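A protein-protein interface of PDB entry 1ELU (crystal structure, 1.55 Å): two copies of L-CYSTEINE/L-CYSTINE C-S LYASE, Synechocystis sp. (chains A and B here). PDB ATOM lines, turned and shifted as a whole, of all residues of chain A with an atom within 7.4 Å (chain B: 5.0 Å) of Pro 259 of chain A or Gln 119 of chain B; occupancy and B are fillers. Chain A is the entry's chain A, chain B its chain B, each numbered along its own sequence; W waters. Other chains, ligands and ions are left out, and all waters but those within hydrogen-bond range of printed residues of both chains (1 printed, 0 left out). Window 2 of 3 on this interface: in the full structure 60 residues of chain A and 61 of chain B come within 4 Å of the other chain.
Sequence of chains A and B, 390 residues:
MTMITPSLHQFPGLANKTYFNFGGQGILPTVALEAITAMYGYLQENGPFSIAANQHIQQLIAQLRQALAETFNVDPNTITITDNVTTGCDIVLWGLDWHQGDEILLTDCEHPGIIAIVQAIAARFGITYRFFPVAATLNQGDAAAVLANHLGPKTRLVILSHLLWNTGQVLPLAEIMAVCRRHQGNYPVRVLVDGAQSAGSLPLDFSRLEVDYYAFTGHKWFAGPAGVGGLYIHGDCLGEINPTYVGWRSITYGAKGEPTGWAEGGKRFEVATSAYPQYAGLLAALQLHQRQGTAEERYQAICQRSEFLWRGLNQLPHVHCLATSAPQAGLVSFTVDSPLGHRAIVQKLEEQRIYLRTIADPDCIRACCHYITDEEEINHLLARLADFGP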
ATOM      1  N   VAL A 246      13.217   1.677 -15.402  1.00  0.00           N
ATOM      2  CA  VAL A 246      14.142   0.738 -14.769  1.00  0.00           C
ATOM      3  C   VAL A 246      14.019   0.825 -13.258  1.00  0.00           C
ATOM      4  O   VAL A 246      13.277   1.653 -12.717  1.00  0.00           O
ATOM      5  CB  VAL A 246      15.623   1.047 -15.130  1.00  0.00           C
ATOM      6  CG1 VAL A 246      15.911   0.693 -16.620  1.00  0.00           C
ATOM      7  CG2 VAL A 246      15.921   2.505 -14.815  1.00  0.00           C
ATOM      8  N   ILE A 251      19.605  -3.444 -13.025  1.00  0.00           N
ATOM      9  CA  ILE A 251      21.033  -3.206 -12.882  1.00  0.00           C
ATOM     10  C   ILE A 251      21.949  -4.286 -12.322  1.00  0.00           C
ATOM     11  O   ILE A 251      21.496  -5.283 -11.756  1.00  0.00           O
ATOM     12  CB  ILE A 251      21.220  -1.979 -11.999  1.00  0.00           C
ATOM     13  CG1 ILE A 251      20.506  -2.188 -10.649  1.00  0.00           C
ATOM     14  CG2 ILE A 251      20.621  -0.786 -12.671  1.00  0.00           C
ATOM     15  CD1 ILE A 251      20.755  -1.060  -9.649  1.00  0.00           C
ATOM     16  N   THR A 252      23.255  -4.054 -12.493  1.00  0.00           N
ATOM     17  CA  THR A 252      24.293  -4.916 -11.920  1.00  0.00           C
ATOM     18  C   THR A 252      24.700  -4.057 -10.722  1.00  0.00           C
ATOM     19  O   THR A 252      24.506  -2.823 -10.735  1.00  0.00           O
ATOM     20  CB  THR A 252      25.522  -5.143 -12.870  1.00  0.00           C
ATOM     21  OG1 THR A 252      25.983  -3.893 -13.401  1.00  0.00           O
ATOM     22  CG2 THR A 252      25.152  -6.083 -14.003  1.00  0.00           C
ATOM     23  N   TYR A 253      25.245  -4.698  -9.684  1.00  0.00           N
ATOM     24  CA  TYR A 253      25.618  -3.984  -8.457  1.00  0.00           C
ATOM     25  C   TYR A 253      27.097  -3.977  -8.083  1.00  0.00           C
ATOM     26  O   TYR A 253      27.809  -4.927  -8.360  1.00  0.00           O
ATOM     27  CB  TYR A 253      24.825  -4.561  -7.273  1.00  0.00           C
ATOM     28  CG  TYR A 253      23.332  -4.337  -7.364  1.00  0.00           C
ATOM     29  CD1 TYR A 253      22.524  -5.170  -8.144  1.00  0.00           C
ATOM     30  CD2 TYR A 253      22.729  -3.295  -6.665  1.00  0.00           C
ATOM     31  CE1 TYR A 253      21.140  -4.961  -8.218  1.00  0.00           C
ATOM     32  CE2 TYR A 253      21.360  -3.079  -6.736  1.00  0.00           C
ATOM     33  CZ  TYR A 253      20.577  -3.918  -7.511  1.00  0.00           C
ATOM     34  OH  TYR A 253      19.235  -3.714  -7.558  1.00  0.00           O
ATOM     35  N   GLY A 254      27.514  -2.895  -7.429  1.00  0.00           N
ATOM     36  CA  GLY A 254      28.892  -2.736  -7.008  1.00  0.00           C
ATOM     37  C   GLY A 254      29.093  -3.073  -5.544  1.00  0.00           C
ATOM     38  O   GLY A 254      28.167  -3.529  -4.862  1.00  0.00           O
ATOM     39  N   LYS A 256      29.330  -1.367  -2.778  1.00  0.00           N
ATOM     40  CA  LYS A 256      28.469  -0.775  -1.772  1.00  0.00           C
ATOM     41  C   LYS A 256      26.981  -0.801  -2.119  1.00  0.00           C
ATOM     42  O   LYS A 256      26.201   0.001  -1.607  1.00  0.00           O
ATOM     43  CB  LYS A 256      28.949   0.647  -1.527  1.00  0.00           C
ATOM     44  CG  LYS A 256      30.402   0.673  -1.077  1.00  0.00           C
ATOM     45  CD  LYS A 256      31.010   2.054  -1.169  1.00  0.00           C
ATOM     46  CE  LYS A 256      30.316   3.039  -0.253  1.00  0.00           C
ATOM     47  NZ  LYS A 256      30.979   4.377  -0.332  1.00  0.00           N
ATOM     48  N   GLY A 257      26.598  -1.729  -2.989  1.00  0.00           N
ATOM     49  CA  GLY A 257      25.207  -1.843  -3.395  1.00  0.00           C
ATOM     50  C   GLY A 257      24.789  -0.808  -4.425  1.00  0.00           C
ATOM     51  O   GLY A 257      23.603  -0.697  -4.743  1.00  0.00           O
ATOM     52  N   GLU A 258      25.750  -0.052  -4.953  1.00  0.00           N
ATOM     53  CA  GLU A 258      25.437   0.977  -5.950  1.00  0.00           C
ATOM     54  C   GLU A 258      25.316   0.410  -7.373  1.00  0.00           C
ATOM     55  O   GLU A 258      25.878  -0.640  -7.691  1.00  0.00           O
ATOM     56  CB  GLU A 258      26.490   2.103  -5.900  1.00  0.00           C
ATOM     57  CG  GLU A 258      27.805   1.837  -6.632  1.00  0.00           C
ATOM     58  CD  GLU A 258      28.748   0.901  -5.909  1.00  0.00           C
ATOM     59  OE1 GLU A 258      28.421   0.436  -4.799  1.00  0.00           O
ATOM     60  OE2 GLU A 258      29.836   0.626  -6.459  1.00  0.00           O
ATOM     61  N   PRO A 259      24.551   1.092  -8.249  1.00  0.00           N
ATOM     62  CA  PRO A 259      24.395   0.601  -9.623  1.00  0.00           C
ATOM     63  C   PRO A 259      25.725   0.697 -10.350  1.00  0.00           C
ATOM     64  O   PRO A 259      26.437   1.698 -10.207  1.00  0.00           O
ATOM     65  CB  PRO A 259      23.368   1.562 -10.245  1.00  0.00           C
ATOM     66  CG  PRO A 259      22.733   2.268  -9.075  1.00  0.00           C
ATOM     67  CD  PRO A 259      23.861   2.377  -8.070  1.00  0.00           C
ATOM     68  N   THR A 260      26.062  -0.327 -11.123  1.00  0.00           N
ATOM     69  CA  THR A 260      27.311  -0.290 -11.886  1.00  0.00           C
ATOM     70  C   THR A 260      27.106  -0.515 -13.379  1.00  0.00           C
ATOM     71  O   THR A 260      28.034  -0.342 -14.170  1.00  0.00           O
ATOM     72  CB  THR A 260      28.323  -1.327 -11.386  1.00  0.00           C
ATOM     73  OG1 THR A 260      27.699  -2.615 -11.316  1.00  0.00           O
ATOM     74  CG2 THR A 260      28.853  -0.926 -10.018  1.00  0.00           C
ATOM     75  N   GLY A 261      25.900  -0.902 -13.768  1.00  0.00           N
ATOM     76  CA  GLY A 261      25.624  -1.124 -15.177  1.00  0.00           C
ATOM     77  C   GLY A 261      24.288  -1.802 -15.398  1.00  0.00           C
ATOM     78  O   GLY A 261      23.515  -1.963 -14.463  1.00  0.00           O
ATOM     79  N   TRP A 262      24.018  -2.203 -16.631  1.00  0.00           N
ATOM     80  CA  TRP A 262      22.760  -2.881 -16.934  1.00  0.00           C
ATOM     81  C   TRP A 262      22.866  -4.393 -16.768  1.00  0.00           C
ATOM     82  O   TRP A 262      23.901  -4.999 -17.109  1.00  0.00           O
ATOM     83  CB  TRP A 262      22.303  -2.587 -18.379  1.00  0.00           C
ATOM     84  CG  TRP A 262      21.960  -1.154 -18.650  1.00  0.00           C
ATOM     85  CD1 TRP A 262      22.433  -0.383 -19.689  1.00  0.00           C
ATOM     86  CD2 TRP A 262      21.106  -0.297 -17.873  1.00  0.00           C
ATOM     87  NE1 TRP A 262      21.931   0.891 -19.592  1.00  0.00           N
ATOM     88  CE2 TRP A 262      21.118   0.973 -18.490  1.00  0.00           C
ATOM     89  CE3 TRP A 262      20.331  -0.477 -16.714  1.00  0.00           C
ATOM     90  CZ2 TRP A 262      20.390   2.053 -17.987  1.00  0.00           C
ATOM     91  CZ3 TRP A 262      19.607   0.592 -16.217  1.00  0.00           C
ATOM     92  CH2 TRP A 262      19.642   1.845 -16.853  1.00  0.00           C
ATOM     93  N   PRO B 112      19.103   2.088  -4.720  1.00  0.00           N
ATOM     94  CA  PRO B 112      19.870   1.969  -5.963  1.00  0.00           C
ATOM     95  C   PRO B 112      19.044   2.003  -7.241  1.00  0.00           C
ATOM     96  O   PRO B 112      19.487   2.548  -8.252  1.00  0.00           O
ATOM     97  CB  PRO B 112      20.618   0.651  -5.789  1.00  0.00           C
ATOM     98  CG  PRO B 112      19.733  -0.145  -4.873  1.00  0.00           C
ATOM     99  CD  PRO B 112      19.307   0.904  -3.866  1.00  0.00           C
ATOM    100  N   ILE B 115      18.288   5.596  -8.093  1.00  0.00           N
ATOM    101  CA  ILE B 115      19.481   6.255  -8.589  1.00  0.00           C
ATOM    102  C   ILE B 115      19.664   5.859 -10.053  1.00  0.00           C
ATOM    103  O   ILE B 115      20.000   6.703 -10.879  1.00  0.00           O
ATOM    104  CB  ILE B 115      20.735   5.847  -7.748  1.00  0.00           C
ATOM    105  CG1 ILE B 115      20.587   6.403  -6.328  1.00  0.00           C
ATOM    106  CG2 ILE B 115      22.006   6.350  -8.409  1.00  0.00           C
ATOM    107  CD1 ILE B 115      21.627   5.881  -5.331  1.00  0.00           C
ATOM    108  N   ALA B 116      19.391   4.594 -10.384  1.00  0.00           N
ATOM    109  CA  ALA B 116      19.557   4.115 -11.750  1.00  0.00           C
ATOM    110  C   ALA B 116      18.617   4.805 -12.739  1.00  0.00           C
ATOM    111  O   ALA B 116      18.957   4.931 -13.919  1.00  0.00           O
ATOM    112  CB  ALA B 116      19.361   2.611 -11.821  1.00  0.00           C
ATOM    113  N   ILE B 117      17.447   5.238 -12.271  1.00  0.00           N
ATOM    114  CA  ILE B 117      16.512   5.936 -13.162  1.00  0.00           C
ATOM    115  C   ILE B 117      17.143   7.290 -13.453  1.00  0.00           C
ATOM    116  O   ILE B 117      17.251   7.686 -14.618  1.00  0.00           O
ATOM    117  CB  ILE B 117      15.133   6.223 -12.529  1.00  0.00           C
ATOM    118  CG1 ILE B 117      14.420   4.920 -12.140  1.00  0.00           C
ATOM    119  CG2 ILE B 117      14.262   6.970 -13.541  1.00  0.00           C
ATOM    120  CD1 ILE B 117      13.177   5.157 -11.277  1.00  0.00           C
ATOM    121  N   VAL B 118      17.577   7.970 -12.388  1.00  0.00           N
ATOM    122  CA  VAL B 118      18.193   9.294 -12.487  1.00  0.00           C
ATOM    123  C   VAL B 118      19.397   9.268 -13.427  1.00  0.00           C
ATOM    124  O   VAL B 118      19.657  10.239 -14.146  1.00  0.00           O
ATOM    125  CB  VAL B 118      18.628   9.819 -11.095  1.00  0.00           C
ATOM    126  CG1 VAL B 118      19.372  11.180 -11.226  1.00  0.00           C
ATOM    127  CG2 VAL B 118      17.399   9.997 -10.192  1.00  0.00           C
ATOM    128  N   GLN B 119      20.126   8.156 -13.425  1.00  0.00           N
ATOM    129  CA  GLN B 119      21.292   8.018 -14.268  1.00  0.00           C
ATOM    130  C   GLN B 119      20.882   7.861 -15.719  1.00  0.00           C
ATOM    131  O   GLN B 119      21.508   8.442 -16.615  1.00  0.00           O
ATOM    132  CB  GLN B 119      22.175   6.852 -13.775  1.00  0.00           C
ATOM    133  CG  GLN B 119      22.787   7.148 -12.387  1.00  0.00           C
ATOM    134  CD  GLN B 119      23.661   6.017 -11.839  1.00  0.00           C
ATOM    135  OE1 GLN B 119      23.459   4.849 -12.157  1.00  0.00           O
ATOM    136  NE2 GLN B 119      24.622   6.367 -10.987  1.00  0.00           N
ATOM    137  N   ALA B 120      19.814   7.106 -15.954  1.00  0.00           N
ATOM    138  CA  ALA B 120      19.325   6.922 -17.317  1.00  0.00           C
ATOM    139  C   ALA B 120      18.800   8.273 -17.836  1.00  0.00           C
ATOM    140  O   ALA B 120      18.962   8.589 -19.015  1.00  0.00           O
ATOM    141  CB  ALA B 120      18.215   5.853 -17.360  1.00  0.00           C
ATOM    142  N   ILE B 121      18.183   9.061 -16.958  1.00  0.00           N
ATOM    143  CA  ILE B 121      17.669  10.378 -17.327  1.00  0.00           C
ATOM    144  C   ILE B 121      18.834  11.322 -17.636  1.00  0.00           C
ATOM    145  O   ILE B 121      18.782  12.081 -18.610  1.00  0.00           O
ATOM    146  CB  ILE B 121      16.857  11.028 -16.203  1.00  0.00           C
ATOM    147  CG1 ILE B 121      15.652  10.160 -15.841  1.00  0.00           C
ATOM    148  CG2 ILE B 121      16.415  12.420 -16.638  1.00  0.00           C
ATOM    149  CD1 ILE B 121      14.581  10.168 -16.848  1.00  0.00           C
ATOM    150  N   ALA B 122      19.870  11.288 -16.792  1.00  0.00           N
ATOM    151  CA  ALA B 122      21.046  12.135 -16.998  1.00  0.00           C
ATOM    152  C   ALA B 122      21.608  11.854 -18.386  1.00  0.00           C
ATOM    153  O   ALA B 122      21.876  12.775 -19.162  1.00  0.00           O
ATOM    154  CB  ALA B 122      22.101  11.845 -15.934  1.00  0.00           C
ATOM    155  N   ALA B 123      21.788  10.589 -18.702  1.00  0.00           N
ATOM    156  CA  ALA B 123      22.314  10.220 -20.007  1.00  0.00           C
ATOM    157  C   ALA B 123      21.432  10.641 -21.185  1.00  0.00           C
ATOM    158  O   ALA B 123      21.937  11.035 -22.244  1.00  0.00           O
ATOM    159  CB  ALA B 123      22.541   8.734 -20.074  1.00  0.00           C
ATOM    160  N   TYR B 129      23.139  15.326 -11.570  1.00  0.00           N
ATOM    161  CA  TYR B 129      22.640  15.036 -10.235  1.00  0.00           C
ATOM    162  C   TYR B 129      23.766  14.970  -9.209  1.00  0.00           C
ATOM    163  O   TYR B 129      24.900  14.613  -9.525  1.00  0.00           O
ATOM    164  CB  TYR B 129      21.884  13.708 -10.241  1.00  0.00           C
ATOM    165  CG  TYR B 129      22.786  12.519 -10.458  1.00  0.00           C
ATOM    166  CD1 TYR B 129      23.357  11.850  -9.376  1.00  0.00           C
ATOM    167  CD2 TYR B 129      23.084  12.070 -11.745  1.00  0.00           C
ATOM    168  CE1 TYR B 129      24.204  10.763  -9.572  1.00  0.00           C
ATOM    169  CE2 TYR B 129      23.931  10.981 -11.952  1.00  0.00           C
ATOM    170  CZ  TYR B 129      24.483  10.337 -10.858  1.00  0.00           C
ATOM    171  OH  TYR B 129      25.312   9.264 -11.061  1.00  0.00           O
HETATM  172  O   HOH W   1      26.384   4.224  -9.401  1.00  0.00           O
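The side-chain amide nitrogen of Gln 119 of chain B is in hydrogen-bond range of the side-chain hydroxyl of Tyr 129 of chain B (3.0 Å).
Among the printed residues, merely in contact across the chains: Val 246 of chain A with Ala 116 of chain B, Val 246 of chain A with Ile 117 of chain B, Ile 251 of chain A with Ala 116 of chain B, Tyr 253 of chain A with Pro 112 of chain B, Gly 257 of chain A with Pro 112 of chain B, Pro 259 of chain A with Pro 112 of chain B and Pro 259 of chain A with Gln 119 of chain B.
Of the printed residues of chain B, Gly 257 of chain A touches Pro 112.
Of chain B, only Pro 112 (3.4 Å) and Gln 119 (3.8 Å) come within 4 Å of Pro 259 of chain A.
Of the printed residues of chain A, Ala 116 of chain B touches Val 246 (3.99 Å) and Ile 251 (3.7 Å).
Of chain A, only Pro 259 (3.8 Å) comes within 4 Å of Gln 119 of chain B.
The nearest residue of chain B that does not touch Pro 259 of chain A is Ile 115 of chain B (4.2 Å).
Hydrophobic or aromatic side chains of chain B within 4 Å of the printed part of chain A: Pro 112, Ala 116 and Ile 117.
Printed residues of chain A that touch a printed residue of chain B: Val 246, Ile 251, Tyr 253, Gly 257 and Pro 259.
Among the printed residues, no Asp or Glu carboxylate lies within 4 Å of a Lys or Arg side-chain nitrogen of the other chain.
No position is printed for both chains.
Of the 7 pairs that touch across the chains among the printed residues, none has its exchanged pair printed and touching as well.
Water W1 bridges the backbone carbonyl oxygen of Pro 259 of chain A (2.7 Å) and the side-chain amide nitrogen of Gln 119 of chain B (3.2 Å).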
